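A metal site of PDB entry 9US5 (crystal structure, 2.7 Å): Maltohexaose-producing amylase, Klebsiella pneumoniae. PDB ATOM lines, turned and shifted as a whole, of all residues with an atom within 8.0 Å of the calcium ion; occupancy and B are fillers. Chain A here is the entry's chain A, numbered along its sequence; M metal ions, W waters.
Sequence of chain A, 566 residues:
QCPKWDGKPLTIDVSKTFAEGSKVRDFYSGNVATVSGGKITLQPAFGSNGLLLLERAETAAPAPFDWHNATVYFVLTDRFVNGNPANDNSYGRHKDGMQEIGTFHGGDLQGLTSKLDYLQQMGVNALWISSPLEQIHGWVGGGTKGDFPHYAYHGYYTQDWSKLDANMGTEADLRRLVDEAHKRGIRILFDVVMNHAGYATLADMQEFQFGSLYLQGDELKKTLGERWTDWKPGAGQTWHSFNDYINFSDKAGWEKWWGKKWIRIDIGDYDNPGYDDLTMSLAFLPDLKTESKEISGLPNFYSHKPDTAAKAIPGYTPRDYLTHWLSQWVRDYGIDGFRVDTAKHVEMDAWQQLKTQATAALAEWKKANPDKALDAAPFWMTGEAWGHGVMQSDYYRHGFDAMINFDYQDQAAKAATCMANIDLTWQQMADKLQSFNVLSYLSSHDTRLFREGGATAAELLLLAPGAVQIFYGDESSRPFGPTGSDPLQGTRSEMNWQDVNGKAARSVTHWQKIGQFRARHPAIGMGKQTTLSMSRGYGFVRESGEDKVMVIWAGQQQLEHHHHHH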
ATOM      1  N   THR A  77       2.794  32.391 -19.265  1.00  0.00           N
ATOM      2  CA  THR A  77       3.193  30.962 -19.228  1.00  0.00           C
ATOM      3  C   THR A  77       1.975  30.100 -18.912  1.00  0.00           C
ATOM      4  O   THR A  77       1.869  29.012 -19.507  1.00  0.00           O
ATOM      5  CB  THR A  77       4.334  30.731 -18.222  1.00  0.00           C
ATOM      6  OG1 THR A  77       5.319  31.732 -18.424  1.00  0.00           O
ATOM      7  CG2 THR A  77       4.943  29.357 -18.395  1.00  0.00           C
ATOM      8  N   ASP A  78       1.081  30.563 -18.029  1.00  0.00           N
ATOM      9  CA  ASP A  78      -0.107  29.776 -17.595  1.00  0.00           C
ATOM     10  C   ASP A  78      -1.038  29.528 -18.786  1.00  0.00           C
ATOM     11  O   ASP A  78      -1.750  28.500 -18.771  1.00  0.00           O
ATOM     12  CB  ASP A  78      -0.891  30.453 -16.470  1.00  0.00           C
ATOM     13  CG  ASP A  78      -2.128  29.658 -16.121  1.00  0.00           C
ATOM     14  OD1 ASP A  78      -1.983  28.479 -15.746  1.00  0.00           O
ATOM     15  OD2 ASP A  78      -3.249  30.194 -16.291  1.00  0.00           O
ATOM     16  N   VAL A  81       1.277  26.609 -22.823  1.00  0.00           N
ATOM     17  CA  VAL A  81       1.345  25.123 -22.946  1.00  0.00           C
ATOM     18  C   VAL A  81       1.473  24.477 -21.559  1.00  0.00           C
ATOM     19  O   VAL A  81       2.369  24.885 -20.785  1.00  0.00           O
ATOM     20  CB  VAL A  81       2.505  24.698 -23.873  1.00  0.00           C
ATOM     21  CG1 VAL A  81       2.679  23.191 -23.926  1.00  0.00           C
ATOM     22  CG2 VAL A  81       2.298  25.253 -25.274  1.00  0.00           C
ATOM     23  N   ASN A  82       0.607  23.495 -21.288  1.00  0.00           N
ATOM     24  CA  ASN A  82       0.595  22.670 -20.050  1.00  0.00           C
ATOM     25  C   ASN A  82       1.407  21.394 -20.291  1.00  0.00           C
ATOM     26  O   ASN A  82       0.813  20.352 -20.649  1.00  0.00           O
ATOM     27  CB  ASN A  82      -0.846  22.372 -19.617  1.00  0.00           C
ATOM     28  CG  ASN A  82      -0.955  21.706 -18.258  1.00  0.00           C
ATOM     29  OD1 ASN A  82       0.047  21.419 -17.612  1.00  0.00           O
ATOM     30  ND2 ASN A  82      -2.173  21.456 -17.815  1.00  0.00           N
ATOM     31  N   GLY A  83       2.731  21.484 -20.143  1.00  0.00           N
ATOM     32  CA  GLY A  83       3.662  20.361 -20.363  1.00  0.00           C
ATOM     33  C   GLY A  83       3.477  19.279 -19.323  1.00  0.00           C
ATOM     34  O   GLY A  83       3.437  18.089 -19.715  1.00  0.00           O
ATOM     35  N   ASN A  84       3.332  19.683 -18.060  1.00  0.00           N
ATOM     36  CA  ASN A  84       3.189  18.822 -16.861  1.00  0.00           C
ATOM     37  C   ASN A  84       1.867  19.150 -16.151  1.00  0.00           C
ATOM     38  O   ASN A  84       1.772  20.162 -15.467  1.00  0.00           O
ATOM     39  CB  ASN A  84       4.370  19.011 -15.915  1.00  0.00           C
ATOM     40  CG  ASN A  84       4.189  18.356 -14.559  1.00  0.00           C
ATOM     41  OD1 ASN A  84       3.326  17.491 -14.387  1.00  0.00           O
ATOM     42  ND2 ASN A  84       4.995  18.756 -13.596  1.00  0.00           N
ATOM     43  N   PRO A  85       0.821  18.305 -16.293  1.00  0.00           N
ATOM     44  CA  PRO A  85      -0.467  18.575 -15.637  1.00  0.00           C
ATOM     45  C   PRO A  85      -0.528  18.330 -14.117  1.00  0.00           C
ATOM     46  O   PRO A  85      -1.528  18.682 -13.517  1.00  0.00           O
ATOM     47  CB  PRO A  85      -1.430  17.590 -16.341  1.00  0.00           C
ATOM     48  CG  PRO A  85      -0.540  16.462 -16.808  1.00  0.00           C
ATOM     49  CD  PRO A  85       0.794  17.101 -17.127  1.00  0.00           C
ATOM     50  N   ALA A  86       0.536  17.757 -13.540  1.00  0.00           N
ATOM     51  CA  ALA A  86       0.612  17.371 -12.105  1.00  0.00           C
ATOM     52  C   ALA A  86       0.691  18.618 -11.215  1.00  0.00           C
ATOM     53  O   ALA A  86       0.300  18.493 -10.034  1.00  0.00           O
ATOM     54  CB  ALA A  86       1.808  16.479 -11.866  1.00  0.00           C
ATOM     55  N   ASN A  87       1.179  19.746 -11.730  1.00  0.00           N
ATOM     56  CA  ASN A  87       1.448  20.976 -10.918  1.00  0.00           C
ATOM     57  C   ASN A  87       0.309  22.000 -11.061  1.00  0.00           C
ATOM     58  O   ASN A  87       0.406  23.048 -10.406  1.00  0.00           O
ATOM     59  CB  ASN A  87       2.794  21.602 -11.289  1.00  0.00           C
ATOM     60  CG  ASN A  87       2.926  21.943 -12.754  1.00  0.00           C
ATOM     61  OD1 ASN A  87       1.923  22.055 -13.462  1.00  0.00           O
ATOM     62  ND2 ASN A  87       4.144  22.117 -13.227  1.00  0.00           N
ATOM     63  N   ASP A  88      -0.741  21.685 -11.830  1.00  0.00           N
ATOM     64  CA  ASP A  88      -1.863  22.616 -12.156  1.00  0.00           C
ATOM     65  C   ASP A  88      -2.609  23.071 -10.896  1.00  0.00           C
ATOM     66  O   ASP A  88      -3.236  24.153 -10.966  1.00  0.00           O
ATOM     67  CB  ASP A  88      -2.846  21.956 -13.116  1.00  0.00           C
ATOM     68  CG  ASP A  88      -2.249  21.635 -14.471  1.00  0.00           C
ATOM     69  OD1 ASP A  88      -1.019  21.774 -14.615  1.00  0.00           O
ATOM     70  OD2 ASP A  88      -3.013  21.251 -15.368  1.00  0.00           O
ATOM     71  N   ASN A  89      -2.543  22.313  -9.796  1.00  0.00           N
ATOM     72  CA  ASN A  89      -3.374  22.543  -8.570  1.00  0.00           C
ATOM     73  C   ASN A  89      -2.493  22.765  -7.334  1.00  0.00           C
ATOM     74  O   ASN A  89      -2.979  22.477  -6.217  1.00  0.00           O
ATOM     75  CB  ASN A  89      -4.331  21.367  -8.353  1.00  0.00           C
ATOM     76  CG  ASN A  89      -5.185  21.113  -9.571  1.00  0.00           C
ATOM     77  OD1 ASN A  89      -4.925  20.183 -10.339  1.00  0.00           O
ATOM     78  ND2 ASN A  89      -6.181  21.964  -9.790  1.00  0.00           N
ATOM     79  N   SER A  90      -1.283  23.294  -7.502  1.00  0.00           N
ATOM     80  CA  SER A  90      -0.348  23.614  -6.391  1.00  0.00           C
ATOM     81  C   SER A  90      -1.064  24.482  -5.350  1.00  0.00           C
ATOM     82  O   SER A  90      -1.913  25.290  -5.754  1.00  0.00           O
ATOM     83  CB  SER A  90       0.895  24.297  -6.882  1.00  0.00           C
ATOM     84  OG  SER A  90       1.507  23.557  -7.912  1.00  0.00           O
ATOM     85  N   LYS A  95      -9.640  25.097 -10.515  1.00  0.00           N
ATOM     86  CA  LYS A  95     -10.403  25.601 -11.684  1.00  0.00           C
ATOM     87  C   LYS A  95     -11.792  26.008 -11.177  1.00  0.00           C
ATOM     88  O   LYS A  95     -12.235  25.447 -10.157  1.00  0.00           O
ATOM     89  CB  LYS A  95     -10.473  24.512 -12.764  1.00  0.00           C
ATOM     90  CG  LYS A  95      -9.127  23.985 -13.268  1.00  0.00           C
ATOM     91  CD  LYS A  95      -8.644  24.623 -14.561  1.00  0.00           C
ATOM     92  CE  LYS A  95      -7.918  23.664 -15.474  1.00  0.00           C
ATOM     93  NZ  LYS A  95      -6.636  23.192 -14.896  1.00  0.00           N
ATOM     94  N   PHE A 104      -5.680  29.421 -12.787  1.00  0.00           N
ATOM     95  CA  PHE A 104      -4.531  28.744 -13.435  1.00  0.00           C
ATOM     96  C   PHE A 104      -5.097  27.671 -14.388  1.00  0.00           C
ATOM     97  O   PHE A 104      -5.786  26.750 -13.922  1.00  0.00           O
ATOM     98  CB  PHE A 104      -3.582  28.125 -12.406  1.00  0.00           C
ATOM     99  CG  PHE A 104      -2.710  29.098 -11.653  1.00  0.00           C
ATOM    100  CD1 PHE A 104      -3.196  29.794 -10.555  1.00  0.00           C
ATOM    101  CD2 PHE A 104      -1.393  29.291 -12.036  1.00  0.00           C
ATOM    102  CE1 PHE A 104      -2.377  30.680  -9.869  1.00  0.00           C
ATOM    103  CE2 PHE A 104      -0.582  30.172 -11.339  1.00  0.00           C
ATOM    104  CZ  PHE A 104      -1.070  30.869 -10.261  1.00  0.00           C
ATOM    105  N   HIS A 105      -4.833  27.810 -15.687  1.00  0.00           N
ATOM    106  CA  HIS A 105      -5.187  26.830 -16.750  1.00  0.00           C
ATOM    107  C   HIS A 105      -4.212  25.660 -16.724  1.00  0.00           C
ATOM    108  O   HIS A 105      -4.555  24.591 -17.266  1.00  0.00           O
ATOM    109  CB  HIS A 105      -5.204  27.505 -18.117  1.00  0.00           C
ATOM    110  CG  HIS A 105      -6.321  28.475 -18.302  1.00  0.00           C
ATOM    111  ND1 HIS A 105      -6.876  28.714 -19.533  1.00  0.00           N
ATOM    112  CD2 HIS A 105      -6.991  29.240 -17.417  1.00  0.00           C
ATOM    113  CE1 HIS A 105      -7.839  29.606 -19.403  1.00  0.00           C
ATOM    114  NE2 HIS A 105      -7.929  29.946 -18.115  1.00  0.00           N
ATOM    115  N   GLY A 106      -3.014  25.857 -16.171  1.00  0.00           N
ATOM    116  CA  GLY A 106      -2.020  24.796 -15.974  1.00  0.00           C
ATOM    117  C   GLY A 106      -0.801  24.938 -16.861  1.00  0.00           C
ATOM    118  O   GLY A 106       0.073  24.060 -16.792  1.00  0.00           O
ATOM    119  N   GLY A 107      -0.720  26.003 -17.670  1.00  0.00           N
ATOM    120  CA  GLY A 107       0.466  26.270 -18.511  1.00  0.00           C
ATOM    121  C   GLY A 107       1.685  26.460 -17.639  1.00  0.00           C
ATOM    122  O   GLY A 107       1.520  27.018 -16.533  1.00  0.00           O
ATOM    123  N   ASP A 108       2.854  25.990 -18.076  1.00  0.00           N
ATOM    124  CA  ASP A 108       4.044  25.867 -17.194  1.00  0.00           C
ATOM    125  C   ASP A 108       5.322  25.989 -18.016  1.00  0.00           C
ATOM    126  O   ASP A 108       5.233  25.993 -19.253  1.00  0.00           O
ATOM    127  CB  ASP A 108       3.987  24.560 -16.400  1.00  0.00           C
ATOM    128  CG  ASP A 108       3.723  23.335 -17.253  1.00  0.00           C
ATOM    129  OD1 ASP A 108       4.394  23.174 -18.292  1.00  0.00           O
ATOM    130  OD2 ASP A 108       2.833  22.544 -16.856  1.00  0.00           O
ATOM    131  N   LEU A 109       6.476  26.069 -17.330  1.00  0.00           N
ATOM    132  CA  LEU A 109       7.812  26.295 -17.945  1.00  0.00           C
ATOM    133  C   LEU A 109       8.175  25.099 -18.836  1.00  0.00           C
ATOM    134  O   LEU A 109       8.790  25.312 -19.896  1.00  0.00           O
ATOM    135  CB  LEU A 109       8.842  26.483 -16.834  1.00  0.00           C
ATOM    136  CG  LEU A 109       8.624  27.702 -15.946  1.00  0.00           C
ATOM    137  CD1 LEU A 109       9.635  27.724 -14.805  1.00  0.00           C
ATOM    138  CD2 LEU A 109       8.698  28.995 -16.742  1.00  0.00           C
ATOM    139  N   GLN A 110       7.829  23.887 -18.415  1.00  0.00           N
ATOM    140  CA  GLN A 110       8.104  22.643 -19.178  1.00  0.00           C
ATOM    141  C   GLN A 110       7.412  22.727 -20.538  1.00  0.00           C
ATOM    142  O   GLN A 110       8.082  22.477 -21.558  1.00  0.00           O
ATOM    143  CB  GLN A 110       7.634  21.440 -18.354  1.00  0.00           C
ATOM    144  CG  GLN A 110       7.994  20.094 -18.955  1.00  0.00           C
ATOM    145  CD  GLN A 110       7.433  19.000 -18.081  1.00  0.00           C
ATOM    146  OE1 GLN A 110       7.728  18.929 -16.884  1.00  0.00           O
ATOM    147  NE2 GLN A 110       6.576  18.169 -18.652  1.00  0.00           N
ATOM    148  N   GLY A 111       6.121  23.087 -20.544  1.00  0.00           N
ATOM    149  CA  GLY A 111       5.305  23.248 -21.761  1.00  0.00           C
ATOM    150  C   GLY A 111       5.861  24.320 -22.685  1.00  0.00           C
ATOM    151  O   GLY A 111       5.892  24.093 -23.916  1.00  0.00           O
ATOM    152  N   ALA A 166       5.030  26.810  -7.674  1.00  0.00           N
ATOM    153  CA  ALA A 166       4.937  25.343  -7.892  1.00  0.00           C
ATOM    154  C   ALA A 166       4.171  25.056  -9.180  1.00  0.00           C
ATOM    155  O   ALA A 166       4.480  24.020  -9.823  1.00  0.00           O
ATOM    156  CB  ALA A 166       4.297  24.691  -6.694  1.00  0.00           C
ATOM    157  N   ASN A 167       3.226  25.929  -9.563  1.00  0.00           N
ATOM    158  CA  ASN A 167       2.441  25.831 -10.817  1.00  0.00           C
ATOM    159  C   ASN A 167       3.353  25.970 -12.046  1.00  0.00           C
ATOM    160  O   ASN A 167       3.025  25.388 -13.086  1.00  0.00           O
ATOM    161  CB  ASN A 167       1.296  26.858 -10.889  1.00  0.00           C
ATOM    162  CG  ASN A 167      -0.048  26.277 -10.498  1.00  0.00           C
ATOM    163  OD1 ASN A 167      -0.371  26.172  -9.324  1.00  0.00           O
ATOM    164  ND2 ASN A 167      -0.847  25.903 -11.492  1.00  0.00           N
ATOM    165  N   MET A 168       4.449  26.728 -11.919  1.00  0.00           N
ATOM    166  CA  MET A 168       5.361  27.050 -13.056  1.00  0.00           C
ATOM    167  C   MET A 168       6.372  25.907 -13.234  1.00  0.00           C
ATOM    168  O   MET A 168       6.672  25.569 -14.401  1.00  0.00           O
ATOM    169  CB  MET A 168       6.091  28.371 -12.808  1.00  0.00           C
ATOM    170  CG  MET A 168       5.170  29.572 -12.940  1.00  0.00           C
ATOM    171  SD  MET A 168       4.358  29.625 -14.560  1.00  0.00           S
ATOM    172  CE  MET A 168       2.675  29.973 -14.067  1.00  0.00           C
ATOM    173  N   GLY A 169       6.862  25.357 -12.131  1.00  0.00           N
ATOM    174  CA  GLY A 169       7.714  24.162 -12.113  1.00  0.00           C
ATOM    175  C   GLY A 169       8.807  24.251 -11.080  1.00  0.00           C
ATOM    176  O   GLY A 169       8.670  25.029 -10.114  1.00  0.00           O
HETATM  177 CA    CA M   1       0.984  22.406 -15.559  1.00  0.00          CA
HETATM  178  O   HOH W   1       0.774  24.453 -14.181  1.00  0.00           O
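N of Gly 106 lies within hydrogen-bond range of OD1 of Asp 78 (2.8 Å).
The side-chain carboxylate of Asp 108 sits at hydrogen-bond distance from the backbone NH of Gly 83, 3.0 Å away.
The backbone NH (N) of Asp 108 is in hydrogen-bond range of the backbone carbonyl oxygen (O) of Val 81.
OD1 of Asp 108 is in hydrogen-bond range of N of Gly 111 (2.8 Å).
O of Asp 88 is in hydrogen-bond range of ND2 of Asn 167 (3.0 Å).
ND2 of Asn 167 sits close to O of Asn 87 (3.3 Å).
OG of Ser 90 lies within hydrogen-bond range of O of Asn 87, at 2.8 Å.
The side-chain amide oxygen (OD1) of Asn 84 is in hydrogen-bond range of the backbone NH (N) of Ala 86 (2.9 Å).
Within 4 Å of the calcium ion: Asn 82, Asn 84, Asn 87, Asp 88, Gly 106 and Asp 108.
The calcium ion is bound by the backbone carbonyl oxygen (O) of Gly 106, the side-chain carboxylate (OD2) of Asp 108, the side-chain carboxylate (OD1) of Asp 88, the side-chain amide oxygen (OD1) of Asn 87, the backbone carbonyl oxygen (O) of Asn 84, the side-chain amide oxygen (OD1) of Asn 82 and water W1.
The calcium ion has seven donor atoms within binding distance.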
